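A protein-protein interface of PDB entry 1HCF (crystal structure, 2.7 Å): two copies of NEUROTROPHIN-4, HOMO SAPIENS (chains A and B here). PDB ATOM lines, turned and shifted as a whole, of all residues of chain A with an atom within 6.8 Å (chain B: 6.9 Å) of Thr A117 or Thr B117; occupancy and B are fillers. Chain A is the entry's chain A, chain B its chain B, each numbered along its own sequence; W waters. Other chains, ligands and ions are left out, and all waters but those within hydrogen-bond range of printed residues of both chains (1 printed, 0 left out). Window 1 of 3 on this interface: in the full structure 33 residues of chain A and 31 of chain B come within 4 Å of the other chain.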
ATOM      1  N   SER A  21      12.883 -14.677 -25.764  1.00  0.00           N
ATOM      2  CA  SER A  21      13.169 -15.848 -24.945  1.00  0.00           C
ATOM      3  C   SER A  21      12.193 -16.976 -25.210  1.00  0.00           C
ATOM      4  O   SER A  21      11.078 -16.752 -25.677  1.00  0.00           O
ATOM      5  CB  SER A  21      13.115 -15.498 -23.461  1.00  0.00           C
ATOM      6  OG  SER A  21      14.197 -14.666 -23.088  1.00  0.00           O
ATOM      7  N   PHE A  57      16.085 -22.629 -20.932  1.00  0.00           N
ATOM      8  CA  PHE A  57      15.514 -21.306 -21.130  1.00  0.00           C
ATOM      9  C   PHE A  57      16.560 -20.505 -21.895  1.00  0.00           C
ATOM     10  O   PHE A  57      17.571 -20.115 -21.327  1.00  0.00           O
ATOM     11  CB  PHE A  57      15.246 -20.645 -19.782  1.00  0.00           C
ATOM     12  CG  PHE A  57      14.477 -19.369 -19.885  1.00  0.00           C
ATOM     13  CD1 PHE A  57      13.107 -19.388 -20.129  1.00  0.00           C
ATOM     14  CD2 PHE A  57      15.123 -18.141 -19.751  1.00  0.00           C
ATOM     15  CE1 PHE A  57      12.385 -18.195 -20.238  1.00  0.00           C
ATOM     16  CE2 PHE A  57      14.420 -16.949 -19.859  1.00  0.00           C
ATOM     17  CZ  PHE A  57      13.042 -16.974 -20.103  1.00  0.00           C
ATOM     18  N   GLU A  58      16.331 -20.262 -23.178  1.00  0.00           N
ATOM     19  CA  GLU A  58      17.312 -19.520 -23.956  1.00  0.00           C
ATOM     20  C   GLU A  58      16.810 -18.189 -24.473  1.00  0.00           C
ATOM     21  O   GLU A  58      15.614 -18.001 -24.683  1.00  0.00           O
ATOM     22  CB  GLU A  58      17.831 -20.389 -25.102  1.00  0.00           C
ATOM     23  CG  GLU A  58      18.503 -21.658 -24.583  1.00  0.00           C
ATOM     24  CD  GLU A  58      19.252 -22.439 -25.647  1.00  0.00           C
ATOM     25  OE1 GLU A  58      20.195 -21.880 -26.267  1.00  0.00           O
ATOM     26  OE2 GLU A  58      18.897 -23.620 -25.851  1.00  0.00           O
ATOM     27  N   THR A  59      17.741 -17.258 -24.653  1.00  0.00           N
ATOM     28  CA  THR A  59      17.419 -15.921 -25.130  1.00  0.00           C
ATOM     29  C   THR A  59      18.288 -15.555 -26.326  1.00  0.00           C
ATOM     30  O   THR A  59      19.503 -15.465 -26.200  1.00  0.00           O
ATOM     31  CB  THR A  59      17.669 -14.887 -24.040  1.00  0.00           C
ATOM     32  OG1 THR A  59      17.064 -15.323 -22.821  1.00  0.00           O
ATOM     33  CG2 THR A  59      17.084 -13.556 -24.440  1.00  0.00           C
ATOM     34  N   ARG A  60      17.667 -15.343 -27.481  1.00  0.00           N
ATOM     35  CA  ARG A  60      18.404 -14.984 -28.685  1.00  0.00           C
ATOM     36  C   ARG A  60      18.024 -13.562 -29.096  1.00  0.00           C
ATOM     37  O   ARG A  60      17.064 -13.001 -28.578  1.00  0.00           O
ATOM     38  CB  ARG A  60      18.061 -15.952 -29.823  1.00  0.00           C
ATOM     39  CG  ARG A  60      16.636 -15.782 -30.364  1.00  0.00           C
ATOM     40  CD  ARG A  60      16.298 -16.773 -31.474  1.00  0.00           C
ATOM     41  NE  ARG A  60      14.870 -16.782 -31.790  1.00  0.00           N
ATOM     42  CZ  ARG A  60      14.197 -15.740 -32.276  1.00  0.00           C
ATOM     43  NH1 ARG A  60      14.818 -14.588 -32.514  1.00  0.00           N
ATOM     44  NH2 ARG A  60      12.890 -15.843 -32.509  1.00  0.00           N
ATOM     45  N   ALA A  92      24.476 -12.210 -29.404  1.00  0.00           N
ATOM     46  CA  ALA A  92      24.018 -13.111 -28.370  1.00  0.00           C
ATOM     47  C   ALA A  92      25.129 -13.265 -27.348  1.00  0.00           C
ATOM     48  O   ALA A  92      26.293 -13.445 -27.702  1.00  0.00           O
ATOM     49  CB  ALA A  92      23.662 -14.467 -28.964  1.00  0.00           C
ATOM     50  N   LYS A  93      24.763 -13.175 -26.078  1.00  0.00           N
ATOM     51  CA  LYS A  93      25.717 -13.334 -24.996  1.00  0.00           C
ATOM     52  C   LYS A  93      25.378 -14.702 -24.420  1.00  0.00           C
ATOM     53  O   LYS A  93      24.205 -15.007 -24.191  1.00  0.00           O
ATOM     54  CB  LYS A  93      25.519 -12.216 -23.962  1.00  0.00           C
ATOM     55  CG  LYS A  93      26.539 -12.163 -22.840  1.00  0.00           C
ATOM     56  CD  LYS A  93      26.224 -13.163 -21.750  1.00  0.00           C
ATOM     57  CE  LYS A  93      27.283 -13.170 -20.652  1.00  0.00           C
ATOM     58  NZ  LYS A  93      27.013 -14.245 -19.653  1.00  0.00           N
ATOM     59  N   GLN A  94      26.399 -15.529 -24.216  1.00  0.00           N
ATOM     60  CA  GLN A  94      26.211 -16.875 -23.677  1.00  0.00           C
ATOM     61  C   GLN A  94      26.565 -16.966 -22.206  1.00  0.00           C
ATOM     62  O   GLN A  94      27.392 -16.213 -21.701  1.00  0.00           O
ATOM     63  CB  GLN A  94      27.060 -17.887 -24.438  1.00  0.00           C
ATOM     64  CG  GLN A  94      26.736 -18.001 -25.909  1.00  0.00           C
ATOM     65  CD  GLN A  94      27.339 -19.250 -26.540  1.00  0.00           C
ATOM     66  OE1 GLN A  94      28.560 -19.398 -26.605  1.00  0.00           O
ATOM     67  NE2 GLN A  94      26.477 -20.165 -26.999  1.00  0.00           N
ATOM     68  N   SER A  95      25.930 -17.908 -21.524  1.00  0.00           N
ATOM     69  CA  SER A  95      26.167 -18.135 -20.107  1.00  0.00           C
ATOM     70  C   SER A  95      26.300 -19.647 -19.959  1.00  0.00           C
ATOM     71  O   SER A  95      25.900 -20.382 -20.850  1.00  0.00           O
ATOM     72  CB  SER A  95      24.972 -17.619 -19.297  1.00  0.00           C
ATOM     73  OG  SER A  95      25.381 -17.001 -18.087  1.00  0.00           O
ATOM     74  N   TYR A  96      26.876 -20.111 -18.856  1.00  0.00           N
ATOM     75  CA  TYR A  96      27.030 -21.543 -18.619  1.00  0.00           C
ATOM     76  C   TYR A  96      25.926 -22.071 -17.708  1.00  0.00           C
ATOM     77  O   TYR A  96      25.615 -21.453 -16.696  1.00  0.00           O
ATOM     78  CB  TYR A  96      28.370 -21.845 -17.948  1.00  0.00           C
ATOM     79  CG  TYR A  96      29.558 -21.833 -18.865  1.00  0.00           C
ATOM     80  CD1 TYR A  96      29.750 -22.848 -19.807  1.00  0.00           C
ATOM     81  CD2 TYR A  96      30.502 -20.804 -18.794  1.00  0.00           C
ATOM     82  CE1 TYR A  96      30.855 -22.841 -20.656  1.00  0.00           C
ATOM     83  CE2 TYR A  96      31.609 -20.786 -19.639  1.00  0.00           C
ATOM     84  CZ  TYR A  96      31.777 -21.804 -20.566  1.00  0.00           C
ATOM     85  OH  TYR A  96      32.857 -21.762 -21.414  1.00  0.00           O
ATOM     86  N   VAL A  97      25.336 -23.203 -18.085  1.00  0.00           N
ATOM     87  CA  VAL A  97      24.306 -23.854 -17.283  1.00  0.00           C
ATOM     88  C   VAL A  97      24.699 -25.306 -17.209  1.00  0.00           C
ATOM     89  O   VAL A  97      25.401 -25.814 -18.083  1.00  0.00           O
ATOM     90  CB  VAL A  97      22.886 -23.795 -17.907  1.00  0.00           C
ATOM     91  CG1 VAL A  97      22.407 -22.374 -17.985  1.00  0.00           C
ATOM     92  CG2 VAL A  97      22.879 -24.449 -19.270  1.00  0.00           C
ATOM     93  N   ILE A 115      24.973 -21.797 -23.356  1.00  0.00           N
ATOM     94  CA  ILE A 115      23.728 -21.491 -24.050  1.00  0.00           C
ATOM     95  C   ILE A 115      23.567 -19.970 -24.188  1.00  0.00           C
ATOM     96  O   ILE A 115      24.271 -19.203 -23.532  1.00  0.00           O
ATOM     97  CB  ILE A 115      22.516 -22.068 -23.278  1.00  0.00           C
ATOM     98  CG1 ILE A 115      22.409 -21.409 -21.902  1.00  0.00           C
ATOM     99  CG2 ILE A 115      22.672 -23.583 -23.114  1.00  0.00           C
ATOM    100  CD1 ILE A 115      21.060 -21.606 -21.226  1.00  0.00           C
ATOM    101  N   ASP A 116      22.659 -19.537 -25.059  1.00  0.00           N
ATOM    102  CA  ASP A 116      22.419 -18.111 -25.244  1.00  0.00           C
ATOM    103  C   ASP A 116      21.443 -17.658 -24.167  1.00  0.00           C
ATOM    104  O   ASP A 116      20.405 -18.291 -23.958  1.00  0.00           O
ATOM    105  CB  ASP A 116      21.818 -17.836 -26.622  1.00  0.00           C
ATOM    106  CG  ASP A 116      22.627 -18.452 -27.747  1.00  0.00           C
ATOM    107  OD1 ASP A 116      23.866 -18.277 -27.776  1.00  0.00           O
ATOM    108  OD2 ASP A 116      22.018 -19.113 -28.617  1.00  0.00           O
ATOM    109  N   THR A 117      21.771 -16.571 -23.476  1.00  0.00           N
ATOM    110  CA  THR A 117      20.888 -16.075 -22.432  1.00  0.00           C
ATOM    111  C   THR A 117      20.599 -14.588 -22.529  1.00  0.00           C
ATOM    112  O   THR A 117      19.883 -14.040 -21.692  1.00  0.00           O
ATOM    113  CB  THR A 117      21.447 -16.361 -21.025  1.00  0.00           C
ATOM    114  OG1 THR A 117      22.709 -15.707 -20.872  1.00  0.00           O
ATOM    115  CG2 THR A 117      21.614 -17.857 -20.810  1.00  0.00           C
ATOM    116  N   ALA A 118      21.143 -13.932 -23.547  1.00  0.00           N
ATOM    117  CA  ALA A 118      20.909 -12.505 -23.710  1.00  0.00           C
ATOM    118  C   ALA A 118      21.433 -11.962 -25.016  1.00  0.00           C
ATOM    119  O   ALA A 118      22.249 -12.587 -25.686  1.00  0.00           O
ATOM    120  CB  ALA A 118      21.547 -11.733 -22.558  1.00  0.00           C
ATOM    121  N   CYS A 119      20.941 -10.783 -25.368  1.00  0.00           N
ATOM    122  CA  CYS A 119      21.375 -10.094 -26.563  1.00  0.00           C
ATOM    123  C   CYS A 119      21.969  -8.767 -26.071  1.00  0.00           C
ATOM    124  O   CYS A 119      21.262  -7.900 -25.551  1.00  0.00           O
ATOM    125  CB  CYS A 119      20.195  -9.856 -27.504  1.00  0.00           C
ATOM    126  SG  CYS A 119      20.716  -9.119 -29.087  1.00  0.00           S
ATOM    127  N   SER B  21      31.691 -12.229 -14.412  1.00  0.00           N
ATOM    128  CA  SER B  21      31.096 -13.544 -14.269  1.00  0.00           C
ATOM    129  C   SER B  21      31.854 -14.316 -13.202  1.00  0.00           C
ATOM    130  O   SER B  21      32.991 -13.988 -12.874  1.00  0.00           O
ATOM    131  CB  SER B  21      31.143 -14.284 -15.604  1.00  0.00           C
ATOM    132  OG  SER B  21      30.363 -13.611 -16.584  1.00  0.00           O
ATOM    133  N   PHE B  57      26.457 -20.250 -12.418  1.00  0.00           N
ATOM    134  CA  PHE B  57      27.331 -19.375 -13.167  1.00  0.00           C
ATOM    135  C   PHE B  57      26.555 -18.083 -13.346  1.00  0.00           C
ATOM    136  O   PHE B  57      25.619 -18.022 -14.139  1.00  0.00           O
ATOM    137  CB  PHE B  57      27.632 -19.966 -14.535  1.00  0.00           C
ATOM    138  CG  PHE B  57      28.634 -19.186 -15.302  1.00  0.00           C
ATOM    139  CD1 PHE B  57      29.991 -19.263 -14.971  1.00  0.00           C
ATOM    140  CD2 PHE B  57      28.232 -18.340 -16.331  1.00  0.00           C
ATOM    141  CE1 PHE B  57      30.934 -18.506 -15.655  1.00  0.00           C
ATOM    142  CE2 PHE B  57      29.171 -17.577 -17.022  1.00  0.00           C
ATOM    143  CZ  PHE B  57      30.528 -17.660 -16.682  1.00  0.00           C
ATOM    144  N   GLU B  58      26.921 -17.047 -12.611  1.00  0.00           N
ATOM    145  CA  GLU B  58      26.200 -15.798 -12.734  1.00  0.00           C
ATOM    146  C   GLU B  58      27.047 -14.670 -13.299  1.00  0.00           C
ATOM    147  O   GLU B  58      28.271 -14.708 -13.247  1.00  0.00           O
ATOM    148  CB  GLU B  58      25.599 -15.417 -11.382  1.00  0.00           C
ATOM    149  CG  GLU B  58      24.604 -16.456 -10.894  1.00  0.00           C
ATOM    150  CD  GLU B  58      23.785 -16.006  -9.697  1.00  0.00           C
ATOM    151  OE1 GLU B  58      23.233 -14.876  -9.733  1.00  0.00           O
ATOM    152  OE2 GLU B  58      23.680 -16.791  -8.723  1.00  0.00           O
ATOM    153  N   THR B  59      26.374 -13.675 -13.863  1.00  0.00           N
ATOM    154  CA  THR B  59      27.032 -12.532 -14.460  1.00  0.00           C
ATOM    155  C   THR B  59      26.305 -11.258 -14.066  1.00  0.00           C
ATOM    156  O   THR B  59      25.113 -11.104 -14.333  1.00  0.00           O
ATOM    157  CB  THR B  59      27.046 -12.652 -15.996  1.00  0.00           C
ATOM    158  OG1 THR B  59      27.758 -13.835 -16.372  1.00  0.00           O
ATOM    159  CG2 THR B  59      27.725 -11.449 -16.623  1.00  0.00           C
ATOM    160  N   ARG B  60      27.037 -10.345 -13.433  1.00  0.00           N
ATOM    161  CA  ARG B  60      26.477  -9.072 -12.990  1.00  0.00           C
ATOM    162  C   ARG B  60      27.185  -7.876 -13.619  1.00  0.00           C
ATOM    163  O   ARG B  60      28.193  -8.021 -14.307  1.00  0.00           O
ATOM    164  CB  ARG B  60      26.568  -8.963 -11.463  1.00  0.00           C
ATOM    165  CG  ARG B  60      25.856 -10.088 -10.732  1.00  0.00           C
ATOM    166  CD  ARG B  60      25.544  -9.741  -9.272  1.00  0.00           C
ATOM    167  NE  ARG B  60      24.568 -10.673  -8.699  1.00  0.00           N
ATOM    168  CZ  ARG B  60      24.824 -11.948  -8.412  1.00  0.00           C
ATOM    169  NH1 ARG B  60      26.034 -12.450  -8.634  1.00  0.00           N
ATOM    170  NH2 ARG B  60      23.864 -12.724  -7.921  1.00  0.00           N
ATOM    171  N   ALA B  92      21.154  -5.282 -14.606  1.00  0.00           N
ATOM    172  CA  ALA B  92      21.351  -6.710 -14.614  1.00  0.00           C
ATOM    173  C   ALA B  92      20.182  -7.279 -15.399  1.00  0.00           C
ATOM    174  O   ALA B  92      19.077  -6.744 -15.374  1.00  0.00           O
ATOM    175  CB  ALA B  92      21.356  -7.253 -13.211  1.00  0.00           C
ATOM    176  N   LYS B  93      20.449  -8.359 -16.112  1.00  0.00           N
ATOM    177  CA  LYS B  93      19.455  -9.026 -16.911  1.00  0.00           C
ATOM    178  C   LYS B  93      19.391 -10.440 -16.355  1.00  0.00           C
ATOM    179  O   LYS B  93      20.419 -11.099 -16.185  1.00  0.00           O
ATOM    180  CB  LYS B  93      19.910  -9.041 -18.370  1.00  0.00           C
ATOM    181  CG  LYS B  93      18.902  -9.632 -19.350  1.00  0.00           C
ATOM    182  CD  LYS B  93      18.901 -11.149 -19.335  1.00  0.00           C
ATOM    183  CE  LYS B  93      17.925 -11.679 -20.370  1.00  0.00           C
ATOM    184  NZ  LYS B  93      17.799 -13.162 -20.362  1.00  0.00           N
ATOM    185  N   GLN B  94      18.189 -10.910 -16.063  1.00  0.00           N
ATOM    186  CA  GLN B  94      18.049 -12.244 -15.517  1.00  0.00           C
ATOM    187  C   GLN B  94      17.413 -13.221 -16.479  1.00  0.00           C
ATOM    188  O   GLN B  94      16.718 -12.846 -17.419  1.00  0.00           O
ATOM    189  CB  GLN B  94      17.217 -12.204 -14.246  1.00  0.00           C
ATOM    190  CG  GLN B  94      17.717 -11.218 -13.254  1.00  0.00           C
ATOM    191  CD  GLN B  94      17.064 -11.396 -11.918  1.00  0.00           C
ATOM    192  OE1 GLN B  94      15.851 -11.264 -11.784  1.00  0.00           O
ATOM    193  NE2 GLN B  94      17.868 -11.700 -10.908  1.00  0.00           N
ATOM    194  N   SER B  95      17.667 -14.493 -16.239  1.00  0.00           N
ATOM    195  CA  SER B  95      17.069 -15.523 -17.059  1.00  0.00           C
ATOM    196  C   SER B  95      16.813 -16.656 -16.098  1.00  0.00           C
ATOM    197  O   SER B  95      17.175 -16.568 -14.927  1.00  0.00           O
ATOM    198  CB  SER B  95      18.014 -15.957 -18.172  1.00  0.00           C
ATOM    199  OG  SER B  95      19.146 -16.587 -17.634  1.00  0.00           O
ATOM    200  N   TYR B  96      16.190 -17.714 -16.586  1.00  0.00           N
ATOM    201  CA  TYR B  96      15.887 -18.855 -15.748  1.00  0.00           C
ATOM    202  C   TYR B  96      16.823 -20.037 -15.972  1.00  0.00           C
ATOM    203  O   TYR B  96      17.294 -20.267 -17.090  1.00  0.00           O
ATOM    204  CB  TYR B  96      14.459 -19.317 -16.017  1.00  0.00           C
ATOM    205  CG  TYR B  96      13.396 -18.358 -15.562  1.00  0.00           C
ATOM    206  CD1 TYR B  96      13.031 -18.285 -14.221  1.00  0.00           C
ATOM    207  CD2 TYR B  96      12.735 -17.538 -16.472  1.00  0.00           C
ATOM    208  CE1 TYR B  96      12.031 -17.420 -13.799  1.00  0.00           C
ATOM    209  CE2 TYR B  96      11.737 -16.667 -16.057  1.00  0.00           C
ATOM    210  CZ  TYR B  96      11.392 -16.616 -14.718  1.00  0.00           C
ATOM    211  OH  TYR B  96      10.408 -15.753 -14.297  1.00  0.00           O
ATOM    212  N   VAL B  97      17.103 -20.761 -14.893  1.00  0.00           N
ATOM    213  CA  VAL B  97      17.899 -21.982 -14.953  1.00  0.00           C
ATOM    214  C   VAL B  97      17.182 -22.893 -13.985  1.00  0.00           C
ATOM    215  O   VAL B  97      16.689 -22.430 -12.960  1.00  0.00           O
ATOM    216  CB  VAL B  97      19.380 -21.808 -14.509  1.00  0.00           C
ATOM    217  CG1 VAL B  97      20.171 -21.154 -15.604  1.00  0.00           C
ATOM    218  CG2 VAL B  97      19.466 -20.995 -13.242  1.00  0.00           C
ATOM    219  N   ILE B 115      18.305 -15.927 -12.121  1.00  0.00           N
ATOM    220  CA  ILE B 115      19.657 -15.564 -11.700  1.00  0.00           C
ATOM    221  C   ILE B 115      20.174 -14.502 -12.677  1.00  0.00           C
ATOM    222  O   ILE B 115      19.615 -14.317 -13.761  1.00  0.00           O
ATOM    223  CB  ILE B 115      20.615 -16.774 -11.747  1.00  0.00           C
ATOM    224  CG1 ILE B 115      20.719 -17.288 -13.185  1.00  0.00           C
ATOM    225  CG2 ILE B 115      20.114 -17.887 -10.818  1.00  0.00           C
ATOM    226  CD1 ILE B 115      21.741 -18.400 -13.392  1.00  0.00           C
ATOM    227  N   ASP B 116      21.229 -13.794 -12.300  1.00  0.00           N
ATOM    228  CA  ASP B 116      21.779 -12.786 -13.193  1.00  0.00           C
ATOM    229  C   ASP B 116      22.664 -13.458 -14.222  1.00  0.00           C
ATOM    230  O   ASP B 116      23.595 -14.173 -13.856  1.00  0.00           O
ATOM    231  CB  ASP B 116      22.598 -11.777 -12.414  1.00  0.00           C
ATOM    232  CG  ASP B 116      21.793 -11.092 -11.361  1.00  0.00           C
ATOM    233  OD1 ASP B 116      20.648 -10.714 -11.668  1.00  0.00           O
ATOM    234  OD2 ASP B 116      22.303 -10.929 -10.234  1.00  0.00           O
ATOM    235  N   THR B 117      22.376 -13.237 -15.503  1.00  0.00           N
ATOM    236  CA  THR B 117      23.177 -13.850 -16.562  1.00  0.00           C
ATOM    237  C   THR B 117      23.785 -12.848 -17.516  1.00  0.00           C
ATOM    238  O   THR B 117      24.445 -13.229 -18.481  1.00  0.00           O
ATOM    239  CB  THR B 117      22.354 -14.821 -17.408  1.00  0.00           C
ATOM    240  OG1 THR B 117      21.239 -14.120 -17.977  1.00  0.00           O
ATOM    241  CG2 THR B 117      21.867 -15.983 -16.556  1.00  0.00           C
ATOM    242  N   ALA B 118      23.562 -11.568 -17.255  1.00  0.00           N
ATOM    243  CA  ALA B 118      24.101 -10.541 -18.119  1.00  0.00           C
ATOM    244  C   ALA B 118      23.872  -9.146 -17.587  1.00  0.00           C
ATOM    245  O   ALA B 118      23.050  -8.927 -16.698  1.00  0.00           O
ATOM    246  CB  ALA B 118      23.495 -10.663 -19.500  1.00  0.00           C
ATOM    247  N   CYS B 119      24.633  -8.205 -18.133  1.00  0.00           N
ATOM    248  CA  CYS B 119      24.507  -6.804 -17.779  1.00  0.00           C
ATOM    249  C   CYS B 119      24.111  -6.142 -19.100  1.00  0.00           C
ATOM    250  O   CYS B 119      24.836  -6.255 -20.079  1.00  0.00           O
ATOM    251  CB  CYS B 119      25.844  -6.247 -17.262  1.00  0.00           C
ATOM    252  SG  CYS B 119      25.723  -4.474 -16.841  1.00  0.00           S
HETATM  253  O   HOH W   1      18.953 -20.841 -18.822  1.00  0.00           O
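Hydrophobic or aromatic side chains of chain B that line the printed part of chain A: Phe B57, Tyr B96, Val B97 and Ala B118.
Along chain B the printed residues that touch a printed residue of chain A span positions 57 to 118.
Hydrophobic or aromatic side chains of chain A within 4 Å of the printed part of chain B: Phe A57, Tyr A96, Val A97 and Ala A118.
Among the printed residues, no Asp or Glu carboxylate lies within 4 Å of a Lys or Arg side-chain nitrogen of the other chain.
O of Thr A117 is in hydrogen-bond range of NZ of Lys B93 (2.6 Å).
The side-chain amino group of Lys B93 lies within hydrogen-bond range of the side-chain hydroxyl of Thr A59.
The side-chain hydroxyl of Thr B59 sits at hydrogen-bond distance from the side-chain amino group of Lys A93, at 3.4 Å.
The backbone carbonyl oxygen (O) of Thr B117 lies within hydrogen-bond range of the side-chain amino group (NZ) of Lys A93, 3.0 Å away.
Thr A117 touches just these residues of chain B: Lys B93 (2.6 Å) and Thr B117 (3.6 Å).
Thr B117 touches just these residues of chain A: Lys A93, Ser A95 and Thr A117.
Printed residues of chain A within 4 Å of Ser B95: Phe A57.
Printed residues of chain A within 4 Å of Thr B59: Lys A93 (3.4 Å).
The nearest printed residue of chain B that does not touch Ala A118 is Lys B93 (4.2 Å).
Phe A57 touches Tyr B96, and with the chains exchanged Tyr A96 touches Phe B57.
Val B97 touches its own counterpart, Val A97.
Thr B117 touches its own counterpart, Thr A117.
Ala A118 touches its own counterpart, Ala B118.
Positions printed for both chains: 21, 57, 58, 59, 60, 92, 93, 94, 95, 96, 97, 115, 116, 117, 118 and 119.
Of the 12 pairs that touch across the chains among the printed residues, 11 have their exchanged pair printed and touching as well.
The backbone carbonyl oxygen (O) of Ile A115 lies within hydrogen-bond range of the backbone NH (N) of Ser A95.
The backbone carbonyl oxygen (O) of Asp A116 sits at hydrogen-bond distance from the backbone NH (N) of Thr A59, at 2.9 Å.
The backbone NH (N) of Thr B59 sits at hydrogen-bond distance from the backbone carbonyl oxygen (O) of Asp B116 (2.8 Å).
The backbone carbonyl oxygen (O) of Ala A118 lies within hydrogen-bond range of the backbone NH (N) of Lys A93 (2.6 Å).
The backbone carbonyl oxygen (O) of Thr A59 is in hydrogen-bond range of the backbone NH (N) of Ala A118 (3.5 Å).
The backbone carbonyl oxygen (O) of Ala B118 sits at hydrogen-bond distance from the backbone NH (N) of Lys B93.
Water W1 lies within hydrogen-bond range of O of Tyr B96 and O of Phe A57.
Among the printed residues, merely in contact across the chains: Tyr A96 with Phe B57 (3.3 Å), Phe A57 with Tyr B96 (3.4 Å), Val A97 with Val B97 (3.5 Å), Thr A117 with Thr B117 (3.6 Å), Ser A95 with Phe B57 (3.6 Å), Ala A118 with Ala B118 (3.8 Å), Ser A95 with Thr B117 (3.8 Å) and Phe A57 with Ser B95 (3.95 Å).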
